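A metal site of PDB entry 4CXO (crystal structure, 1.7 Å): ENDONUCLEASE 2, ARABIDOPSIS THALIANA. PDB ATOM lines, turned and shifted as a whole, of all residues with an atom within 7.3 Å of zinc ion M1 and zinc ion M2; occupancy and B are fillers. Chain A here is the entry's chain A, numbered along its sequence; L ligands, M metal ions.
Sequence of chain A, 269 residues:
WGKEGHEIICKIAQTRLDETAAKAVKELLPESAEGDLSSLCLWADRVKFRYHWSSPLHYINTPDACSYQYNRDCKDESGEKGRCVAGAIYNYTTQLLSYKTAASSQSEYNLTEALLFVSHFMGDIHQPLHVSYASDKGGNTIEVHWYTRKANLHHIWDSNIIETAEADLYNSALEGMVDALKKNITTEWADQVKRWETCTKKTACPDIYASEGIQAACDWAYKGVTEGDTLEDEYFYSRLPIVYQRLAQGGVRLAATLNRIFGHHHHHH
O4 of LIG L1 is bound to zinc ion M1 (1.9 Å). NE2 of His 6 is bound to zinc ion M1, at 2.0 Å. Zinc ion M1 is bound by N of Trp 1, at 2.0 Å. OD1 of Asp 124 is bound to zinc ion M1 (2.1 Å). O of Trp 1 binds zinc ion M1 (2.3 Å). Zinc ion M1 has five donor atoms within binding distance.
Along chain A the residues within 4 Å of zinc ion M1 span positions 1 to 124. The nearest printed residue that does not touch zinc ion M1 is Gly 2 (4.2 Å).
Along chain A the residues within 4 Å of zinc ion M2 span positions 45 to 124.
An oxygen (O4) of LIG L1 binds zinc ion M2 (2.1 Å). Zinc ion M2 is bound by ND1 of His 58, 2.1 Å away. OD2 of Asp 124 binds zinc ion M2. Zinc ion M2 is bound by NE2 of His 120 (2.2 Å). O2 of LIG L1 is bound to zinc ion M2 (2.4 Å). Zinc ion M2 is bound by OD1 of Asp 45, 2.4 Å away. Zinc ion M2 has six donor atoms within binding distance.
The backbone carbonyl oxygen (O) of Gly 123 sits at hydrogen-bond distance from the indole nitrogen (NE1) of Trp 1, at 2.8 Å. O of His 58 is in hydrogen-bond range of ND1 of His 130, 2.7 Å away. A ring nitrogen (ND1) of His 120 lies within hydrogen-bond range of the backbone carbonyl oxygen of Cys 41. The side-chain amino group (NZ) of Lys 48 sits close to the side-chain carboxylate (OD1) of Asp 45 (3.7 Å).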
ATOM      1  N   TRP A   1       5.775   0.823  13.989  1.00  0.00           N
ATOM      2  CA  TRP A   1       5.643   0.850  15.458  1.00  0.00           C
ATOM      3  C   TRP A   1       4.780   1.973  15.927  1.00  0.00           C
ATOM      4  O   TRP A   1       4.573   2.933  15.219  1.00  0.00           O
ATOM      5  CB  TRP A   1       7.007   1.043  16.111  1.00  0.00           C
ATOM      6  CG  TRP A   1       8.081   0.079  15.690  1.00  0.00           C
ATOM      7  CD1 TRP A   1       9.058   0.317  14.778  1.00  0.00           C
ATOM      8  CD2 TRP A   1       8.332  -1.199  16.228  1.00  0.00           C
ATOM      9  NE1 TRP A   1       9.890  -0.755  14.680  1.00  0.00           N
ATOM     10  CE2 TRP A   1       9.472  -1.716  15.562  1.00  0.00           C
ATOM     11  CE3 TRP A   1       7.687  -1.994  17.173  1.00  0.00           C
ATOM     12  CZ2 TRP A   1       9.985  -2.981  15.828  1.00  0.00           C
ATOM     13  CZ3 TRP A   1       8.202  -3.262  17.457  1.00  0.00           C
ATOM     14  CH2 TRP A   1       9.349  -3.740  16.778  1.00  0.00           C
ATOM     15  N   GLY A   2       4.333   1.874  17.170  1.00  0.00           N
ATOM     16  CA  GLY A   2       3.648   2.969  17.823  1.00  0.00           C
ATOM     17  C   GLY A   2       4.645   3.959  18.382  1.00  0.00           C
ATOM     18  O   GLY A   2       5.839   3.875  18.126  1.00  0.00           O
ATOM     19  N   LYS A   3       4.145   4.905  19.178  1.00  0.00           N
ATOM     20  CA  LYS A   3       4.947   5.994  19.706  1.00  0.00           C
ATOM     21  C   LYS A   3       6.175   5.522  20.466  1.00  0.00           C
ATOM     22  O   LYS A   3       7.269   6.032  20.271  1.00  0.00           O
ATOM     23  CB  LYS A   3       4.069   6.848  20.644  1.00  0.00           C
ATOM     24  CG  LYS A   3       4.788   8.006  21.349  1.00  0.00           C
ATOM     25  CD  LYS A   3       3.846   8.778  22.278  1.00  0.00           C
ATOM     26  CE  LYS A   3       4.558   9.911  22.997  1.00  0.00           C
ATOM     27  N   GLY A   5       7.855   2.648  20.404  1.00  0.00           N
ATOM     28  CA  GLY A   5       8.873   2.020  19.551  1.00  0.00           C
ATOM     29  C   GLY A   5       9.734   3.014  18.784  1.00  0.00           C
ATOM     30  O   GLY A   5      10.978   2.879  18.748  1.00  0.00           O
ATOM     31  N   HIS A   6       9.105   3.986  18.149  1.00  0.00           N
ATOM     32  CA  HIS A   6       9.861   5.012  17.444  1.00  0.00           C
ATOM     33  C   HIS A   6      10.715   5.865  18.368  1.00  0.00           C
ATOM     34  O   HIS A   6      11.835   6.220  18.046  1.00  0.00           O
ATOM     35  CB  HIS A   6       8.932   5.898  16.599  1.00  0.00           C
ATOM     36  CG  HIS A   6       8.369   5.176  15.435  1.00  0.00           C
ATOM     37  ND1 HIS A   6       9.110   4.887  14.309  1.00  0.00           N
ATOM     38  CD2 HIS A   6       7.163   4.597  15.258  1.00  0.00           C
ATOM     39  CE1 HIS A   6       8.357   4.190  13.476  1.00  0.00           C
ATOM     40  NE2 HIS A   6       7.181   3.995  14.038  1.00  0.00           N
ATOM     41  N   CYS A  41       9.859  11.577  15.803  1.00  0.00           N
ATOM     42  CA  CYS A  41       9.958  10.309  15.097  1.00  0.00           C
ATOM     43  C   CYS A  41       8.621   9.637  14.822  1.00  0.00           C
ATOM     44  O   CYS A  41       8.589   8.617  14.164  1.00  0.00           O
ATOM     45  CB  CYS A  41      10.953   9.365  15.777  1.00  0.00           C
ATOM     46  SG  CYS A  41      12.647   9.833  15.322  1.00  0.00           S
ATOM     47  N   LEU A  42       7.528  10.229  15.295  1.00  0.00           N
ATOM     48  CA  LEU A  42       6.196   9.818  14.897  1.00  0.00           C
ATOM     49  C   LEU A  42       5.569  10.778  13.861  1.00  0.00           C
ATOM     50  O   LEU A  42       4.441  10.565  13.411  1.00  0.00           O
ATOM     51  CB  LEU A  42       5.283   9.687  16.118  1.00  0.00           C
ATOM     52  CG  LEU A  42       4.191   8.618  16.063  1.00  0.00           C
ATOM     53  CD1 LEU A  42       4.781   7.215  15.976  1.00  0.00           C
ATOM     54  CD2 LEU A  42       3.309   8.725  17.296  1.00  0.00           C
ATOM     55  N   ALA A  44       5.899  11.246  10.702  1.00  0.00           N
ATOM     56  CA  ALA A  44       5.428  10.598   9.487  1.00  0.00           C
ATOM     57  C   ALA A  44       4.056   9.963   9.658  1.00  0.00           C
ATOM     58  O   ALA A  44       3.236   9.975   8.750  1.00  0.00           O
ATOM     59  CB  ALA A  44       6.430   9.560   9.006  1.00  0.00           C
ATOM     60  N   ASP A  45       3.772   9.399  10.827  1.00  0.00           N
ATOM     61  CA  ASP A  45       2.446   8.825  11.042  1.00  0.00           C
ATOM     62  C   ASP A  45       1.379   9.902  11.053  1.00  0.00           C
ATOM     63  O   ASP A  45       0.230   9.622  10.762  1.00  0.00           O
ATOM     64  CB  ASP A  45       2.376   8.084  12.362  1.00  0.00           C
ATOM     65  CG  ASP A  45       2.784   6.655  12.263  1.00  0.00           C
ATOM     66  OD1 ASP A  45       3.086   6.164  11.147  1.00  0.00           O
ATOM     67  OD2 ASP A  45       2.806   6.020  13.322  1.00  0.00           O
ATOM     68  N   LYS A  48      -0.050  10.768   7.272  1.00  0.00           N
ATOM     69  CA  LYS A  48      -0.593   9.740   6.409  1.00  0.00           C
ATOM     70  C   LYS A  48      -1.816  10.178   5.637  1.00  0.00           C
ATOM     71  O   LYS A  48      -2.057   9.670   4.546  1.00  0.00           O
ATOM     72  CB  LYS A  48      -0.982   8.488   7.200  1.00  0.00           C
ATOM     73  CG  LYS A  48       0.177   7.649   7.654  1.00  0.00           C
ATOM     74  CD  LYS A  48      -0.352   6.460   8.439  1.00  0.00           C
ATOM     75  CE  LYS A  48       0.779   5.616   8.950  1.00  0.00           C
ATOM     76  NZ  LYS A  48       0.316   4.311   9.454  1.00  0.00           N
ATOM     77  N   SER A  55       1.034   6.985   2.657  1.00  0.00           N
ATOM     78  CA  SER A  55       0.512   5.925   3.523  1.00  0.00           C
ATOM     79  C   SER A  55       1.142   4.548   3.237  1.00  0.00           C
ATOM     80  O   SER A  55       1.545   3.844   4.167  1.00  0.00           O
ATOM     81  CB  SER A  55      -1.006   5.859   3.408  1.00  0.00           C
ATOM     82  OG  SER A  55      -1.520   4.860   4.259  1.00  0.00           O
ATOM     83  N   LEU A  57       3.997   3.933   2.104  1.00  0.00           N
ATOM     84  CA  LEU A  57       5.431   3.969   2.348  1.00  0.00           C
ATOM     85  C   LEU A  57       5.819   3.446   3.735  1.00  0.00           C
ATOM     86  O   LEU A  57       6.983   3.279   4.029  1.00  0.00           O
ATOM     87  CB  LEU A  57       5.951   5.405   2.172  1.00  0.00           C
ATOM     88  CG  LEU A  57       5.608   6.039   0.832  1.00  0.00           C
ATOM     89  CD1 LEU A  57       6.209   7.429   0.741  1.00  0.00           C
ATOM     90  CD2 LEU A  57       6.107   5.150  -0.311  1.00  0.00           C
ATOM     91  N   HIS A  58       4.839   3.170   4.581  1.00  0.00           N
ATOM     92  CA  HIS A  58       5.159   2.678   5.926  1.00  0.00           C
ATOM     93  C   HIS A  58       5.409   1.191   5.994  1.00  0.00           C
ATOM     94  O   HIS A  58       5.882   0.702   7.038  1.00  0.00           O
ATOM     95  CB  HIS A  58       4.057   3.046   6.905  1.00  0.00           C
ATOM     96  CG  HIS A  58       3.968   4.515   7.149  1.00  0.00           C
ATOM     97  ND1 HIS A  58       4.283   5.064   8.365  1.00  0.00           N
ATOM     98  CD2 HIS A  58       3.645   5.543   6.337  1.00  0.00           C
ATOM     99  CE1 HIS A  58       4.140   6.377   8.301  1.00  0.00           C
ATOM    100  NE2 HIS A  58       3.748   6.689   7.081  1.00  0.00           N
ATOM    101  N   TYR A  59       5.111   0.473   4.925  1.00  0.00           N
ATOM    102  CA  TYR A  59       5.141  -0.987   4.990  1.00  0.00           C
ATOM    103  C   TYR A  59       5.470  -1.643   3.651  1.00  0.00           C
ATOM    104  O   TYR A  59       5.651  -0.971   2.632  1.00  0.00           O
ATOM    105  CB  TYR A  59       3.812  -1.516   5.541  1.00  0.00           C
ATOM    106  CG  TYR A  59       2.610  -1.111   4.723  1.00  0.00           C
ATOM    107  CD1 TYR A  59       2.260  -1.812   3.577  1.00  0.00           C
ATOM    108  CD2 TYR A  59       1.827  -0.035   5.092  1.00  0.00           C
ATOM    109  CE1 TYR A  59       1.185  -1.433   2.797  1.00  0.00           C
ATOM    110  CE2 TYR A  59       0.744   0.355   4.328  1.00  0.00           C
ATOM    111  CZ  TYR A  59       0.425  -0.352   3.187  1.00  0.00           C
ATOM    112  OH  TYR A  59      -0.639   0.025   2.428  1.00  0.00           O
ATOM    113  N   HIS A 120      11.635   7.748  10.709  1.00  0.00           N
ATOM    114  CA  HIS A 120      10.459   6.944  10.976  1.00  0.00           C
ATOM    115  C   HIS A 120      10.467   5.617  10.205  1.00  0.00           C
ATOM    116  O   HIS A 120      10.161   4.546  10.756  1.00  0.00           O
ATOM    117  CB  HIS A 120       9.207   7.725  10.601  1.00  0.00           C
ATOM    118  CG  HIS A 120       7.945   7.011  10.935  1.00  0.00           C
ATOM    119  ND1 HIS A 120       7.315   7.140  12.149  1.00  0.00           N
ATOM    120  CD2 HIS A 120       7.188   6.158  10.200  1.00  0.00           C
ATOM    121  CE1 HIS A 120       6.218   6.398  12.157  1.00  0.00           C
ATOM    122  NE2 HIS A 120       6.115   5.800  10.984  1.00  0.00           N
ATOM    123  N   PHE A 121      10.762   5.693   8.908  1.00  0.00           N
ATOM    124  CA  PHE A 121      10.756   4.510   8.051  1.00  0.00           C
ATOM    125  C   PHE A 121      11.838   3.506   8.431  1.00  0.00           C
ATOM    126  O   PHE A 121      11.619   2.285   8.351  1.00  0.00           O
ATOM    127  CB  PHE A 121      10.814   4.903   6.584  1.00  0.00           C
ATOM    128  CG  PHE A 121       9.587   5.653   6.110  1.00  0.00           C
ATOM    129  CD1 PHE A 121       8.326   5.337   6.590  1.00  0.00           C
ATOM    130  CD2 PHE A 121       9.696   6.664   5.181  1.00  0.00           C
ATOM    131  CE1 PHE A 121       7.200   6.023   6.157  1.00  0.00           C
ATOM    132  CE2 PHE A 121       8.569   7.350   4.748  1.00  0.00           C
ATOM    133  CZ  PHE A 121       7.318   7.034   5.232  1.00  0.00           C
ATOM    134  N   GLY A 123      12.681   2.921  11.308  1.00  0.00           N
ATOM    135  CA  GLY A 123      12.007   2.200  12.384  1.00  0.00           C
ATOM    136  C   GLY A 123      10.977   1.213  11.873  1.00  0.00           C
ATOM    137  O   GLY A 123      11.011   0.066  12.241  1.00  0.00           O
ATOM    138  N   ASP A 124      10.071   1.678  11.017  1.00  0.00           N
ATOM    139  CA  ASP A 124       8.992   0.821  10.520  1.00  0.00           C
ATOM    140  C   ASP A 124       9.464  -0.410   9.776  1.00  0.00           C
ATOM    141  O   ASP A 124       8.871  -1.480   9.927  1.00  0.00           O
ATOM    142  CB  ASP A 124       8.024   1.625   9.638  1.00  0.00           C
ATOM    143  CG  ASP A 124       6.940   2.293  10.445  1.00  0.00           C
ATOM    144  OD1 ASP A 124       6.947   2.156  11.688  1.00  0.00           O
ATOM    145  OD2 ASP A 124       6.084   2.950   9.815  1.00  0.00           O
ATOM    146  N   ILE A 125      10.557  -0.297   9.036  1.00  0.00           N
ATOM    147  CA  ILE A 125      11.042  -1.451   8.267  1.00  0.00           C
ATOM    148  C   ILE A 125      11.555  -2.528   9.191  1.00  0.00           C
ATOM    149  O   ILE A 125      11.785  -3.640   8.750  1.00  0.00           O
ATOM    150  CB  ILE A 125      12.112  -1.064   7.210  1.00  0.00           C
ATOM    151  CG1 ILE A 125      12.236  -2.164   6.153  1.00  0.00           C
ATOM    152  CG2 ILE A 125      13.450  -0.763   7.850  1.00  0.00           C
ATOM    153  CD1 ILE A 125      12.952  -1.736   4.887  1.00  0.00           C
ATOM    154  N   GLN A 127       9.806  -3.337  12.044  1.00  0.00           N
ATOM    155  CA  GLN A 127       8.657  -3.952  12.702  1.00  0.00           C
ATOM    156  C   GLN A 127       8.320  -5.148  11.820  1.00  0.00           C
ATOM    157  O   GLN A 127       8.011  -4.984  10.654  1.00  0.00           O
ATOM    158  CB  GLN A 127       7.504  -2.955  12.798  1.00  0.00           C
ATOM    159  CG  GLN A 127       6.544  -3.169  13.978  1.00  0.00           C
ATOM    160  CD  GLN A 127       5.549  -4.313  13.785  1.00  0.00           C
ATOM    161  OE1 GLN A 127       5.942  -5.450  13.583  1.00  0.00           O
ATOM    162  NE2 GLN A 127       4.267  -4.009  13.905  1.00  0.00           N
ATOM    163  N   HIS A 130       5.374  -5.067   9.539  1.00  0.00           N
ATOM    164  CA  HIS A 130       5.417  -4.086   8.467  1.00  0.00           C
ATOM    165  C   HIS A 130       6.052  -4.628   7.187  1.00  0.00           C
ATOM    166  O   HIS A 130       6.127  -3.928   6.204  1.00  0.00           O
ATOM    167  CB  HIS A 130       6.165  -2.830   8.927  1.00  0.00           C
ATOM    168  CG  HIS A 130       5.303  -1.891   9.692  1.00  0.00           C
ATOM    169  ND1 HIS A 130       5.054  -0.606   9.268  1.00  0.00           N
ATOM    170  CD2 HIS A 130       4.588  -2.063  10.823  1.00  0.00           C
ATOM    171  CE1 HIS A 130       4.230  -0.017  10.109  1.00  0.00           C
ATOM    172  NE2 HIS A 130       3.917  -0.888  11.052  1.00  0.00           N
ATOM    173  N   HIS A 154      -1.274  -6.995  14.481  1.00  0.00           N
ATOM    174  CA  HIS A 154      -0.397  -5.908  14.079  1.00  0.00           C
ATOM    175  C   HIS A 154      -0.160  -4.915  15.236  1.00  0.00           C
ATOM    176  O   HIS A 154       0.982  -4.526  15.523  1.00  0.00           O
ATOM    177  CB  HIS A 154      -0.937  -5.195  12.854  1.00  0.00           C
ATOM    178  CG  HIS A 154      -0.025  -4.141  12.333  1.00  0.00           C
ATOM    179  ND1 HIS A 154       0.883  -4.374  11.323  1.00  0.00           N
ATOM    180  CD2 HIS A 154       0.197  -2.883  12.758  1.00  0.00           C
ATOM    181  CE1 HIS A 154       1.592  -3.278  11.114  1.00  0.00           C
ATOM    182  NE2 HIS A 154       1.194  -2.358  11.976  1.00  0.00           N
ATOM    183  N   ASP A 158       3.046  -3.401  17.077  1.00  0.00           N
ATOM    184  CA  ASP A 158       3.313  -1.961  17.085  1.00  0.00           C
ATOM    185  C   ASP A 158       3.486  -1.404  18.506  1.00  0.00           C
ATOM    186  O   ASP A 158       4.341  -0.536  18.731  1.00  0.00           O
ATOM    187  CB  ASP A 158       2.175  -1.182  16.421  1.00  0.00           C
ATOM    188  CG  ASP A 158       2.343  -0.993  14.929  1.00  0.00           C
ATOM    189  OD1 ASP A 158       3.404  -1.307  14.342  1.00  0.00           O
ATOM    190  OD2 ASP A 158       1.372  -0.502  14.327  1.00  0.00           O
HETATM  191  S1  LIG L   1       3.032   2.856  12.119  1.00  0.00           S
HETATM  192  O1  LIG L   1       2.029   3.607  12.943  1.00  0.00           O
HETATM  193  O2  LIG L   1       2.648   2.978  10.644  1.00  0.00           O
HETATM  194  O3  LIG L   1       3.007   1.464  12.652  1.00  0.00           O
HETATM  195  O4  LIG L   1       4.387   3.507  12.286  1.00  0.00           O
HETATM  196  P1  LG2 L   2      -4.340   0.916   8.596  1.00  0.00           P
HETATM  197  O1  LG2 L   2      -4.179   1.692   7.319  1.00  0.00           O
HETATM  198  O2  LG2 L   2      -4.991   1.698   9.707  1.00  0.00           O
HETATM  199  O3  LG2 L   2      -4.848  -0.504   8.422  1.00  0.00           O
HETATM  200  O4  LG2 L   2      -2.832   0.703   9.124  1.00  0.00           O
HETATM  201  C1  LG2 L   2      -2.652   0.171  10.434  1.00  0.00           C
HETATM  202  C2  LG2 L   2      -1.210  -0.256  10.651  1.00  0.00           C
HETATM  203  O5  LG2 L   2      -0.819  -1.368   9.847  1.00  0.00           O
HETATM  204  C3  LG2 L   2      -0.206   0.802  10.262  1.00  0.00           C
HETATM  205  O6  LG2 L   2       0.864   0.600  11.175  1.00  0.00           O
HETATM  206  C4  LG2 L   2       0.253   0.481   8.843  1.00  0.00           C
HETATM  207  C5  LG2 L   2       0.237  -1.047   8.911  1.00  0.00           C
HETATM  208  N1  LG2 L   2      -0.067  -1.818   7.692  1.00  0.00           N
HETATM  209  C6  LG2 L   2       0.803  -2.883   7.302  1.00  0.00           C
HETATM  210  O7  LG2 L   2       1.854  -3.117   7.951  1.00  0.00           O
HETATM  211  N2  LG2 L   2       0.520  -3.635   6.225  1.00  0.00           N
HETATM  212  C7  LG2 L   2      -0.574  -3.420   5.504  1.00  0.00           C
HETATM  213  O8  LG2 L   2      -0.810  -4.134   4.513  1.00  0.00           O
HETATM  214  C8  LG2 L   2      -1.511  -2.324   5.892  1.00  0.00           C
HETATM  215  C9  LG2 L   2      -2.762  -2.026   5.131  1.00  0.00           C
HETATM  216  C10 LG2 L   2      -1.201  -1.569   7.007  1.00  0.00           C
HETATM  217 ZN    ZN M   1       5.782   2.749  13.294  1.00  0.00          ZN
HETATM  218 ZN    ZN M   2       4.540   4.350  10.374  1.00  0.00          ZN
HETATM  219 ZN    ZN M   3       2.217  -0.499  12.334  1.00  0.00          ZN
